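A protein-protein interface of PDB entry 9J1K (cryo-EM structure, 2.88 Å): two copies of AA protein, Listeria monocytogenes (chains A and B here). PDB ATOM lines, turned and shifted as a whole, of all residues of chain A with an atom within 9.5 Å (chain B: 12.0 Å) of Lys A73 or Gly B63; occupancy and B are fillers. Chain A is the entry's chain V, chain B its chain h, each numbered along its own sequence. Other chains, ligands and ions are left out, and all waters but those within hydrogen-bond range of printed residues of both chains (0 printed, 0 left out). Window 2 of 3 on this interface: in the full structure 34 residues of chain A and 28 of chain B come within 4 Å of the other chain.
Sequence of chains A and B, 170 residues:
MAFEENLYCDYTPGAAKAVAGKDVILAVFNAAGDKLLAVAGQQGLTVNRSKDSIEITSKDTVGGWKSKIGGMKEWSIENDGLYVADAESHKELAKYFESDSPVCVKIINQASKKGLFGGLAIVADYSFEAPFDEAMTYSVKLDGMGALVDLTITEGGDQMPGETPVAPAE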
ATOM      1  N   ASN A  48       6.976  -5.048   9.638  1.00  0.00           N
ATOM      2  CA  ASN A  48       6.155  -5.865  10.525  1.00  0.00           C
ATOM      3  C   ASN A  48       7.029  -6.446  11.624  1.00  0.00           C
ATOM      4  O   ASN A  48       7.958  -7.213  11.348  1.00  0.00           O
ATOM      5  CB  ASN A  48       5.427  -6.976   9.759  1.00  0.00           C
ATOM      6  CG  ASN A  48       6.214  -7.486   8.571  1.00  0.00           C
ATOM      7  OD1 ASN A  48       7.439  -7.557   8.604  1.00  0.00           O
ATOM      8  ND2 ASN A  48       5.507  -7.844   7.505  1.00  0.00           N
ATOM      9  N   ARG A  49       6.732  -6.070  12.865  1.00  0.00           N
ATOM     10  CA  ARG A  49       7.361  -6.637  14.049  1.00  0.00           C
ATOM     11  C   ARG A  49       6.299  -7.379  14.841  1.00  0.00           C
ATOM     12  O   ARG A  49       5.247  -6.810  15.158  1.00  0.00           O
ATOM     13  CB  ARG A  49       8.009  -5.550  14.910  1.00  0.00           C
ATOM     14  CG  ARG A  49       8.969  -4.649  14.157  1.00  0.00           C
ATOM     15  CD  ARG A  49       9.310  -3.409  14.966  1.00  0.00           C
ATOM     16  NE  ARG A  49       8.121  -2.651  15.334  1.00  0.00           N
ATOM     17  CZ  ARG A  49       8.097  -1.697  16.255  1.00  0.00           C
ATOM     18  NH1 ARG A  49       9.184  -1.360  16.929  1.00  0.00           N
ATOM     19  NH2 ARG A  49       6.954  -1.065  16.505  1.00  0.00           N
ATOM     20  N   SER A  50       6.568  -8.640  15.160  1.00  0.00           N
ATOM     21  CA  SER A  50       5.590  -9.489  15.822  1.00  0.00           C
ATOM     22  C   SER A  50       6.187 -10.074  17.093  1.00  0.00           C
ATOM     23  O   SER A  50       7.403 -10.237  17.209  1.00  0.00           O
ATOM     24  CB  SER A  50       5.115 -10.621  14.904  1.00  0.00           C
ATOM     25  OG  SER A  50       4.825 -11.791  15.649  1.00  0.00           O
ATOM     26  N   LYS A  51       5.313 -10.371  18.052  1.00  0.00           N
ATOM     27  CA  LYS A  51       5.698 -10.993  19.309  1.00  0.00           C
ATOM     28  C   LYS A  51       4.758 -12.150  19.605  1.00  0.00           C
ATOM     29  O   LYS A  51       3.542 -12.035  19.423  1.00  0.00           O
ATOM     30  CB  LYS A  51       5.666  -9.988  20.467  1.00  0.00           C
ATOM     31  CG  LYS A  51       6.315 -10.500  21.743  1.00  0.00           C
ATOM     32  CD  LYS A  51       5.884  -9.690  22.954  1.00  0.00           C
ATOM     33  CE  LYS A  51       5.882  -8.200  22.659  1.00  0.00           C
ATOM     34  NZ  LYS A  51       6.046  -7.392  23.899  1.00  0.00           N
ATOM     35  N   ASP A  52       5.325 -13.262  20.059  1.00  0.00           N
ATOM     36  CA  ASP A  52       4.529 -14.437  20.374  1.00  0.00           C
ATOM     37  C   ASP A  52       3.961 -14.342  21.785  1.00  0.00           C
ATOM     38  O   ASP A  52       4.537 -13.703  22.670  1.00  0.00           O
ATOM     39  CB  ASP A  52       5.368 -15.708  20.236  1.00  0.00           C
ATOM     40  CG  ASP A  52       6.191 -15.725  18.965  1.00  0.00           C
ATOM     41  OD1 ASP A  52       6.025 -14.805  18.136  1.00  0.00           O
ATOM     42  OD2 ASP A  52       7.004 -16.657  18.793  1.00  0.00           O
ATOM     43  N   SER A  53       2.817 -14.988  21.986  1.00  0.00           N
ATOM     44  CA  SER A  53       2.156 -15.045  23.282  1.00  0.00           C
ATOM     45  C   SER A  53       2.078 -16.496  23.731  1.00  0.00           C
ATOM     46  O   SER A  53       1.650 -17.364  22.964  1.00  0.00           O
ATOM     47  CB  SER A  53       0.754 -14.433  23.215  1.00  0.00           C
ATOM     48  OG  SER A  53       0.759 -13.233  22.462  1.00  0.00           O
ATOM     49  N   ILE A  54       2.491 -16.755  24.968  1.00  0.00           N
ATOM     50  CA  ILE A  54       2.496 -18.096  25.536  1.00  0.00           C
ATOM     51  C   ILE A  54       1.378 -18.184  26.565  1.00  0.00           C
ATOM     52  O   ILE A  54       1.255 -17.315  27.439  1.00  0.00           O
ATOM     53  CB  ILE A  54       3.856 -18.444  26.164  1.00  0.00           C
ATOM     54  CG1 ILE A  54       4.955 -18.430  25.101  1.00  0.00           C
ATOM     55  CG2 ILE A  54       3.797 -19.797  26.854  1.00  0.00           C
ATOM     56  CD1 ILE A  54       6.248 -17.806  25.574  1.00  0.00           C
ATOM     57  N   GLY A  70       3.828 -12.434  27.323  1.00  0.00           N
ATOM     58  CA  GLY A  70       4.618 -12.204  26.132  1.00  0.00           C
ATOM     59  C   GLY A  70       5.755 -13.199  26.004  1.00  0.00           C
ATOM     60  O   GLY A  70       6.274 -13.723  26.990  1.00  0.00           O
ATOM     61  N   GLY A  71       6.142 -13.463  24.763  1.00  0.00           N
ATOM     62  CA  GLY A  71       7.195 -14.416  24.465  1.00  0.00           C
ATOM     63  C   GLY A  71       8.220 -13.822  23.519  1.00  0.00           C
ATOM     64  O   GLY A  71       8.555 -12.640  23.582  1.00  0.00           O
ATOM     65  N   MET A  72       8.719 -14.672  22.627  1.00  0.00           N
ATOM     66  CA  MET A  72       9.738 -14.262  21.674  1.00  0.00           C
ATOM     67  C   MET A  72       9.154 -13.293  20.651  1.00  0.00           C
ATOM     68  O   MET A  72       7.952 -13.293  20.378  1.00  0.00           O
ATOM     69  CB  MET A  72      10.319 -15.486  20.966  1.00  0.00           C
ATOM     70  CG  MET A  72      11.536 -16.164  21.628  1.00  0.00           C
ATOM     71  SD  MET A  72      12.655 -15.279  22.749  1.00  0.00           S
ATOM     72  CE  MET A  72      13.024 -13.762  21.871  1.00  0.00           C
ATOM     73  N   LYS A  73      10.022 -12.456  20.083  1.00  0.00           N
ATOM     74  CA  LYS A  73       9.600 -11.485  19.085  1.00  0.00           C
ATOM     75  C   LYS A  73      10.625 -11.415  17.963  1.00  0.00           C
ATOM     76  O   LYS A  73      11.813 -11.682  18.163  1.00  0.00           O
ATOM     77  CB  LYS A  73       9.381 -10.097  19.709  1.00  0.00           C
ATOM     78  CG  LYS A  73      10.571  -9.160  19.631  1.00  0.00           C
ATOM     79  CD  LYS A  73      10.230  -7.805  20.229  1.00  0.00           C
ATOM     80  CE  LYS A  73      10.392  -7.803  21.739  1.00  0.00           C
ATOM     81  NZ  LYS A  73      11.802  -8.037  22.149  1.00  0.00           N
ATOM     82  N   GLU A  74      10.145 -11.051  16.776  1.00  0.00           N
ATOM     83  CA  GLU A  74      10.965 -10.973  15.574  1.00  0.00           C
ATOM     84  C   GLU A  74      10.460  -9.835  14.698  1.00  0.00           C
ATOM     85  O   GLU A  74       9.421  -9.226  14.971  1.00  0.00           O
ATOM     86  CB  GLU A  74      10.963 -12.303  14.809  1.00  0.00           C
ATOM     87  CG  GLU A  74       9.580 -12.898  14.581  1.00  0.00           C
ATOM     88  CD  GLU A  74       8.845 -12.257  13.421  1.00  0.00           C
ATOM     89  OE1 GLU A  74       9.516 -11.771  12.486  1.00  0.00           O
ATOM     90  OE2 GLU A  74       7.597 -12.238  13.444  1.00  0.00           O
ATOM     91  N   TRP A  75      11.207  -9.545  13.631  1.00  0.00           N
ATOM     92  CA  TRP A  75      10.891  -8.399  12.793  1.00  0.00           C
ATOM     93  C   TRP A  75      11.323  -8.642  11.353  1.00  0.00           C
ATOM     94  O   TRP A  75      12.273  -9.387  11.079  1.00  0.00           O
ATOM     95  CB  TRP A  75      11.556  -7.126  13.325  1.00  0.00           C
ATOM     96  CG  TRP A  75      13.023  -7.052  13.049  1.00  0.00           C
ATOM     97  CD1 TRP A  75      14.030  -7.537  13.830  1.00  0.00           C
ATOM     98  CD2 TRP A  75      13.651  -6.447  11.914  1.00  0.00           C
ATOM     99  NE1 TRP A  75      15.247  -7.274  13.250  1.00  0.00           N
ATOM    100  CE2 TRP A  75      15.040  -6.604  12.072  1.00  0.00           C
ATOM    101  CE3 TRP A  75      13.172  -5.789  10.777  1.00  0.00           C
ATOM    102  CZ2 TRP A  75      15.956  -6.129  11.138  1.00  0.00           C
ATOM    103  CZ3 TRP A  75      14.083  -5.318   9.850  1.00  0.00           C
ATOM    104  CH2 TRP A  75      15.459  -5.492  10.035  1.00  0.00           C
ATOM    105  N   SER A  76      10.624  -7.974  10.438  1.00  0.00           N
ATOM    106  CA  SER A  76      10.916  -8.069   9.016  1.00  0.00           C
ATOM    107  C   SER A  76      10.421  -6.806   8.327  1.00  0.00           C
ATOM    108  O   SER A  76       9.628  -6.041   8.884  1.00  0.00           O
ATOM    109  CB  SER A  76      10.272  -9.313   8.396  1.00  0.00           C
ATOM    110  OG  SER A  76      10.254  -9.223   6.983  1.00  0.00           O
ATOM    111  N   GLY A 144      14.989  -9.989  10.035  1.00  0.00           N
ATOM    112  CA  GLY A 144      16.086  -9.564  10.887  1.00  0.00           C
ATOM    113  C   GLY A 144      16.424 -10.575  11.967  1.00  0.00           C
ATOM    114  O   GLY A 144      15.544 -11.246  12.508  1.00  0.00           O
ATOM    115  N   MET A 145      17.714 -10.675  12.268  1.00  0.00           N
ATOM    116  CA  MET A 145      18.202 -11.425  13.413  1.00  0.00           C
ATOM    117  C   MET A 145      18.547 -10.457  14.535  1.00  0.00           C
ATOM    118  O   MET A 145      19.052  -9.357  14.298  1.00  0.00           O
ATOM    119  CB  MET A 145      19.434 -12.259  13.054  1.00  0.00           C
ATOM    120  CG  MET A 145      20.553 -11.478  12.388  1.00  0.00           C
ATOM    121  SD  MET A 145      21.013 -12.143  10.779  1.00  0.00           S
ATOM    122  CE  MET A 145      19.588 -11.668   9.811  1.00  0.00           C
ATOM    123  N   GLY A 146      18.265 -10.874  15.763  1.00  0.00           N
ATOM    124  CA  GLY A 146      18.528  -9.979  16.866  1.00  0.00           C
ATOM    125  C   GLY A 146      17.516  -8.845  16.924  1.00  0.00           C
ATOM    126  O   GLY A 146      16.412  -8.915  16.378  1.00  0.00           O
ATOM    127  N   ALA A 147      17.921  -7.775  17.602  1.00  0.00           N
ATOM    128  CA  ALA A 147      17.036  -6.657  17.882  1.00  0.00           C
ATOM    129  C   ALA A 147      16.984  -5.681  16.714  1.00  0.00           C
ATOM    130  O   ALA A 147      18.001  -5.400  16.074  1.00  0.00           O
ATOM    131  CB  ALA A 147      17.488  -5.922  19.145  1.00  0.00           C
ATOM    132  N   LEU A 148      15.786  -5.173  16.440  1.00  0.00           N
ATOM    133  CA  LEU A 148      15.588  -4.044  15.534  1.00  0.00           C
ATOM    134  C   LEU A 148      15.371  -2.814  16.406  1.00  0.00           C
ATOM    135  O   LEU A 148      14.292  -2.627  16.974  1.00  0.00           O
ATOM    136  CB  LEU A 148      14.408  -4.282  14.600  1.00  0.00           C
ATOM    137  CG  LEU A 148      14.007  -3.100  13.715  1.00  0.00           C
ATOM    138  CD1 LEU A 148      14.947  -2.970  12.529  1.00  0.00           C
ATOM    139  CD2 LEU A 148      12.568  -3.242  13.247  1.00  0.00           C
ATOM    140  N   VAL A 149      16.403  -1.978  16.518  1.00  0.00           N
ATOM    141  CA  VAL A 149      16.329  -0.828  17.405  1.00  0.00           C
ATOM    142  C   VAL A 149      15.301   0.168  16.882  1.00  0.00           C
ATOM    143  O   VAL A 149      14.970   0.195  15.688  1.00  0.00           O
ATOM    144  CB  VAL A 149      17.713  -0.170  17.563  1.00  0.00           C
ATOM    145  CG1 VAL A 149      18.792  -1.233  17.684  1.00  0.00           C
ATOM    146  CG2 VAL A 149      17.998   0.762  16.399  1.00  0.00           C
ATOM    147  N   SER B  53      15.525 -19.371   6.233  1.00  0.00           N
ATOM    148  CA  SER B  53      16.062 -18.668   7.398  1.00  0.00           C
ATOM    149  C   SER B  53      15.995 -19.628   8.581  1.00  0.00           C
ATOM    150  O   SER B  53      14.908 -19.927   9.082  1.00  0.00           O
ATOM    151  CB  SER B  53      15.286 -17.388   7.680  1.00  0.00           C
ATOM    152  OG  SER B  53      14.066 -17.674   8.341  1.00  0.00           O
ATOM    153  N   ILE B  54      17.148 -20.110   9.027  1.00  0.00           N
ATOM    154  CA  ILE B  54      17.188 -21.089  10.105  1.00  0.00           C
ATOM    155  C   ILE B  54      17.221 -20.357  11.438  1.00  0.00           C
ATOM    156  O   ILE B  54      18.069 -19.485  11.663  1.00  0.00           O
ATOM    157  CB  ILE B  54      18.393 -22.032   9.949  1.00  0.00           C
ATOM    158  CG1 ILE B  54      18.075 -23.163   8.965  1.00  0.00           C
ATOM    159  CG2 ILE B  54      18.793 -22.618  11.292  1.00  0.00           C
ATOM    160  CD1 ILE B  54      17.967 -22.731   7.515  1.00  0.00           C
ATOM    161  N   GLU B  55      16.292 -20.708  12.323  1.00  0.00           N
ATOM    162  CA  GLU B  55      16.144 -20.053  13.617  1.00  0.00           C
ATOM    163  C   GLU B  55      17.010 -20.781  14.636  1.00  0.00           C
ATOM    164  O   GLU B  55      16.824 -21.980  14.872  1.00  0.00           O
ATOM    165  CB  GLU B  55      14.670 -20.048  14.027  1.00  0.00           C
ATOM    166  CG  GLU B  55      14.257 -19.029  15.089  1.00  0.00           C
ATOM    167  CD  GLU B  55      14.416 -19.521  16.520  1.00  0.00           C
ATOM    168  OE1 GLU B  55      13.727 -18.968  17.402  1.00  0.00           O
ATOM    169  OE2 GLU B  55      15.202 -20.454  16.772  1.00  0.00           O
ATOM    170  N   ILE B  56      17.951 -20.058  15.240  1.00  0.00           N
ATOM    171  CA  ILE B  56      18.902 -20.658  16.169  1.00  0.00           C
ATOM    172  C   ILE B  56      18.861 -19.976  17.532  1.00  0.00           C
ATOM    173  O   ILE B  56      19.881 -19.887  18.225  1.00  0.00           O
ATOM    174  CB  ILE B  56      20.323 -20.661  15.563  1.00  0.00           C
ATOM    175  CG1 ILE B  56      20.682 -19.331  14.874  1.00  0.00           C
ATOM    176  CG2 ILE B  56      20.474 -21.814  14.583  1.00  0.00           C
ATOM    177  CD1 ILE B  56      20.656 -18.080  15.726  1.00  0.00           C
ATOM    178  N   THR B  57      17.685 -19.492  17.925  1.00  0.00           N
ATOM    179  CA  THR B  57      17.536 -18.866  19.233  1.00  0.00           C
ATOM    180  C   THR B  57      17.754 -19.890  20.341  1.00  0.00           C
ATOM    181  O   THR B  57      17.321 -21.041  20.243  1.00  0.00           O
ATOM    182  CB  THR B  57      16.149 -18.236  19.365  1.00  0.00           C
ATOM    183  OG1 THR B  57      15.914 -17.362  18.253  1.00  0.00           O
ATOM    184  CG2 THR B  57      16.040 -17.440  20.655  1.00  0.00           C
ATOM    185  N   SER B  58      18.432 -19.462  21.403  1.00  0.00           N
ATOM    186  CA  SER B  58      18.715 -20.317  22.548  1.00  0.00           C
ATOM    187  C   SER B  58      18.489 -19.504  23.817  1.00  0.00           C
ATOM    188  O   SER B  58      17.967 -18.385  23.777  1.00  0.00           O
ATOM    189  CB  SER B  58      20.139 -20.882  22.460  1.00  0.00           C
ATOM    190  OG  SER B  58      21.033 -20.118  23.247  1.00  0.00           O
ATOM    191  N   LYS B  59      18.887 -20.067  24.958  1.00  0.00           N
ATOM    192  CA  LYS B  59      18.668 -19.414  26.242  1.00  0.00           C
ATOM    193  C   LYS B  59      19.669 -18.306  26.537  1.00  0.00           C
ATOM    194  O   LYS B  59      19.419 -17.496  27.436  1.00  0.00           O
ATOM    195  CB  LYS B  59      18.708 -20.441  27.375  1.00  0.00           C
ATOM    196  CG  LYS B  59      17.782 -21.626  27.179  1.00  0.00           C
ATOM    197  CD  LYS B  59      17.085 -21.996  28.476  1.00  0.00           C
ATOM    198  CE  LYS B  59      16.269 -23.267  28.322  1.00  0.00           C
ATOM    199  NZ  LYS B  59      16.146 -24.002  29.610  1.00  0.00           N
ATOM    200  N   ASP B  60      20.786 -18.241  25.816  1.00  0.00           N
ATOM    201  CA  ASP B  60      21.788 -17.210  26.048  1.00  0.00           C
ATOM    202  C   ASP B  60      21.609 -15.995  25.149  1.00  0.00           C
ATOM    203  O   ASP B  60      22.421 -15.068  25.217  1.00  0.00           O
ATOM    204  CB  ASP B  60      23.198 -17.783  25.866  1.00  0.00           C
ATOM    205  CG  ASP B  60      23.273 -18.800  24.751  1.00  0.00           C
ATOM    206  OD1 ASP B  60      22.650 -18.573  23.693  1.00  0.00           O
ATOM    207  OD2 ASP B  60      23.959 -19.829  24.930  1.00  0.00           O
ATOM    208  N   THR B  61      20.575 -15.975  24.314  1.00  0.00           N
ATOM    209  CA  THR B  61      20.299 -14.827  23.454  1.00  0.00           C
ATOM    210  C   THR B  61      19.489 -13.817  24.255  1.00  0.00           C
ATOM    211  O   THR B  61      18.278 -13.965  24.425  1.00  0.00           O
ATOM    212  CB  THR B  61      19.557 -15.256  22.194  1.00  0.00           C
ATOM    213  OG1 THR B  61      18.162 -15.403  22.486  1.00  0.00           O
ATOM    214  CG2 THR B  61      20.105 -16.578  21.681  1.00  0.00           C
ATOM    215  N   VAL B  62      20.159 -12.786  24.749  1.00  0.00           N
ATOM    216  CA  VAL B  62      19.521 -11.755  25.558  1.00  0.00           C
ATOM    217  C   VAL B  62      19.021 -10.646  24.646  1.00  0.00           C
ATOM    218  O   VAL B  62      19.541 -10.429  23.546  1.00  0.00           O
ATOM    219  CB  VAL B  62      20.491 -11.211  26.627  1.00  0.00           C
ATOM    220  CG1 VAL B  62      20.700 -12.242  27.724  1.00  0.00           C
ATOM    221  CG2 VAL B  62      21.815 -10.823  25.990  1.00  0.00           C
ATOM    222  N   GLY B  63      17.997  -9.936  25.108  1.00  0.00           N
ATOM    223  CA  GLY B  63      17.399  -8.848  24.357  1.00  0.00           C
ATOM    224  C   GLY B  63      15.951  -9.061  23.976  1.00  0.00           C
ATOM    225  O   GLY B  63      15.301  -8.107  23.523  1.00  0.00           O
ATOM    226  N   GLY B  64      15.408 -10.265  24.140  1.00  0.00           N
ATOM    227  CA  GLY B  64      14.018 -10.497  23.804  1.00  0.00           C
ATOM    228  C   GLY B  64      13.719 -10.529  22.325  1.00  0.00           C
ATOM    229  O   GLY B  64      12.577 -10.285  21.929  1.00  0.00           O
ATOM    230  N   TRP B  65      14.712 -10.829  21.490  1.00  0.00           N
ATOM    231  CA  TRP B  65      14.542 -10.878  20.045  1.00  0.00           C
ATOM    232  C   TRP B  65      15.057 -12.210  19.521  1.00  0.00           C
ATOM    233  O   TRP B  65      16.122 -12.673  19.939  1.00  0.00           O
ATOM    234  CB  TRP B  65      15.286  -9.727  19.365  1.00  0.00           C
ATOM    235  CG  TRP B  65      14.627  -8.397  19.525  1.00  0.00           C
ATOM    236  CD1 TRP B  65      14.799  -7.519  20.552  1.00  0.00           C
ATOM    237  CD2 TRP B  65      13.707  -7.781  18.619  1.00  0.00           C
ATOM    238  NE1 TRP B  65      14.034  -6.396  20.348  1.00  0.00           N
ATOM    239  CE2 TRP B  65      13.355  -6.533  19.166  1.00  0.00           C
ATOM    240  CE3 TRP B  65      13.144  -8.165  17.398  1.00  0.00           C
ATOM    241  CZ2 TRP B  65      12.466  -5.666  18.537  1.00  0.00           C
ATOM    242  CZ3 TRP B  65      12.260  -7.305  16.776  1.00  0.00           C
ATOM    243  CH2 TRP B  65      11.930  -6.070  17.346  1.00  0.00           C
ATOM    244  N   LYS B  66      14.301 -12.821  18.614  1.00  0.00           N
ATOM    245  CA  LYS B  66      14.738 -14.062  17.991  1.00  0.00           C
ATOM    246  C   LYS B  66      15.924 -13.809  17.067  1.00  0.00           C
ATOM    247  O   LYS B  66      16.052 -12.743  16.459  1.00  0.00           O
ATOM    248  CB  LYS B  66      13.595 -14.701  17.204  1.00  0.00           C
ATOM    249  CG  LYS B  66      12.297 -14.837  17.976  1.00  0.00           C
ATOM    250  CD  LYS B  66      11.557 -16.105  17.584  1.00  0.00           C
ATOM    251  CE  LYS B  66      10.093 -15.820  17.290  1.00  0.00           C
ATOM    252  NZ  LYS B  66       9.567 -16.686  16.200  1.00  0.00           N
ATOM    253  N   SER B  67      16.795 -14.809  16.960  1.00  0.00           N
ATOM    254  CA  SER B  67      17.982 -14.736  16.121  1.00  0.00           C
ATOM    255  C   SER B  67      17.921 -15.827  15.062  1.00  0.00           C
ATOM    256  O   SER B  67      17.616 -16.983  15.374  1.00  0.00           O
ATOM    257  CB  SER B  67      19.255 -14.865  16.962  1.00  0.00           C
ATOM    258  OG  SER B  67      19.220 -16.023  17.778  1.00  0.00           O
ATOM    259  N   LYS B  68      18.199 -15.454  13.813  1.00  0.00           N
ATOM    260  CA  LYS B  68      18.145 -16.364  12.678  1.00  0.00           C
ATOM    261  C   LYS B  68      19.388 -16.175  11.818  1.00  0.00           C
ATOM    262  O   LYS B  68      20.088 -15.166  11.918  1.00  0.00           O
ATOM    263  CB  LYS B  68      16.887 -16.140  11.823  1.00  0.00           C
ATOM    264  CG  LYS B  68      15.646 -15.731  12.603  1.00  0.00           C
ATOM    265  CD  LYS B  68      14.396 -16.384  12.031  1.00  0.00           C
ATOM    266  CE  LYS B  68      13.129 -15.735  12.564  1.00  0.00           C
ATOM    267  NZ  LYS B  68      12.781 -14.487  11.832  1.00  0.00           N
ATOM    268  N   ILE B  69      19.664 -17.168  10.970  1.00  0.00           N
ATOM    269  CA  ILE B  69      20.787 -17.099  10.046  1.00  0.00           C
ATOM    270  C   ILE B  69      20.323 -17.578   8.676  1.00  0.00           C
ATOM    271  O   ILE B  69      19.262 -18.190   8.527  1.00  0.00           O
ATOM    272  CB  ILE B  69      22.010 -17.904  10.545  1.00  0.00           C
ATOM    273  CG1 ILE B  69      21.613 -19.294  11.048  1.00  0.00           C
ATOM    274  CG2 ILE B  69      22.710 -17.151  11.668  1.00  0.00           C
ATOM    275  CD1 ILE B  69      21.470 -20.329   9.954  1.00  0.00           C
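The side-chain carboxylate (OD2) of Asp A52 is in salt-bridge range of the side-chain amino group (NZ) of Lys B66. The backbone carbonyl oxygen of Lys A73 sits at hydrogen-bond distance from the backbone NH of Lys B66, 2.8 Å away. The backbone NH (N) of Gly A146 sits at hydrogen-bond distance from the backbone carbonyl oxygen (O) of Lys B66 (3.0 Å). The side-chain amino group of Lys A73 lies close to the backbone carbonyl oxygen of Gly B64, at 2.4 Å. The side-chain amino group (NZ) of Lys A73 lies close to the indole nitrogen (NE1) of Trp B65 (3.3 Å). O of Lys B68 sits close to SD of Met A145 (3.4 Å).
The backbone NH (N) of Glu A74 lies within hydrogen-bond range of the backbone carbonyl oxygen (O) of Ser A50 (2.9 Å). N of Gly A71 lies within hydrogen-bond range of O of Asp A52, 2.6 Å away. O of Met A72 sits at hydrogen-bond distance from N of Asp A52, at 2.6 Å. O of Trp A75 sits at hydrogen-bond distance from N of Gly A144, at 3.0 Å. N of Ile B56 lies within hydrogen-bond range of O of Ser B67 (3.1 Å). OG1 of Thr B57 sits at hydrogen-bond distance from N of Ser B67, 3.0 Å away.
Gly B64 touches Met A72 (C to CE, 3.3 Å). CE of Met A72 touches N of Trp B65, 3.4 Å away. CE of Met A72 touches N of Lys B66 (3.6 Å). NZ of Lys A73 touches O of Gly B63 (3.8 Å). Glu A74 touches Trp B65. O of Lys B66 touches C of Met A145, at 3.9 Å. O of Gly A146 touches CB of Trp B65, 3.3 Å away. N of Gly A146 touches CA of Ser B67 (3.9 Å). CG of Trp B65 touches CA of Ala A147, at 3.4 Å. Leu A148 touches Trp B65.
Lys A73 touches just these residues of chain B: Gly B63 (3.8 Å), Gly B64 (2.4 Å), Trp B65 (3.3 Å) and Lys B66 (2.8 Å). Of chain A, only Lys A73 comes within 4 Å of Gly B63. Asp A52 touches one residue of chain B. Gly A146 touches just these residues of chain B: Trp B65, Lys B66 and Ser B67. Gly B64 touches just these residues of chain A: Met A72 and Lys A73. Of the printed residues of chain B, Leu A148 touches Trp B65. Printed residues of chain A within 4 Å of Lys B68: Met A145. Printed residues of chain A within 4 Å of Lys B66: Asp A52 (3.5 Å), Met A72 (3.6 Å), Lys A73 (2.8 Å), Met A145 (3.9 Å) and Gly A146 (3.0 Å). The nearest residue of chain A that does not touch Gly B63 is Ala A147 (5.4 Å).
Of the 20 printed residues of chain A, 9 touch a printed residue of chain B. Hydrophobic or aromatic side chains of chain A within 4 Å of the printed part of chain B: Met A72, Trp A75, Met A145 and Ala A147. Of the 17 printed residues of chain B, 6 touch a printed residue of chain A. Hydrophobic or aromatic side chains of chain B that line the printed part of chain A: Trp B65. Among the printed residues, 17 pairs touch across the chains. Among the printed residues, Asp or Glu carboxylates within 4 Å of a Lys or Arg side-chain nitrogen of the other chain: Asp A52 with Lys B66.
Positions printed for both chains: 53 and 54. Of the 17 pairs that touch across the chains among the printed residues, none has its exchanged pair printed and touching as well.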
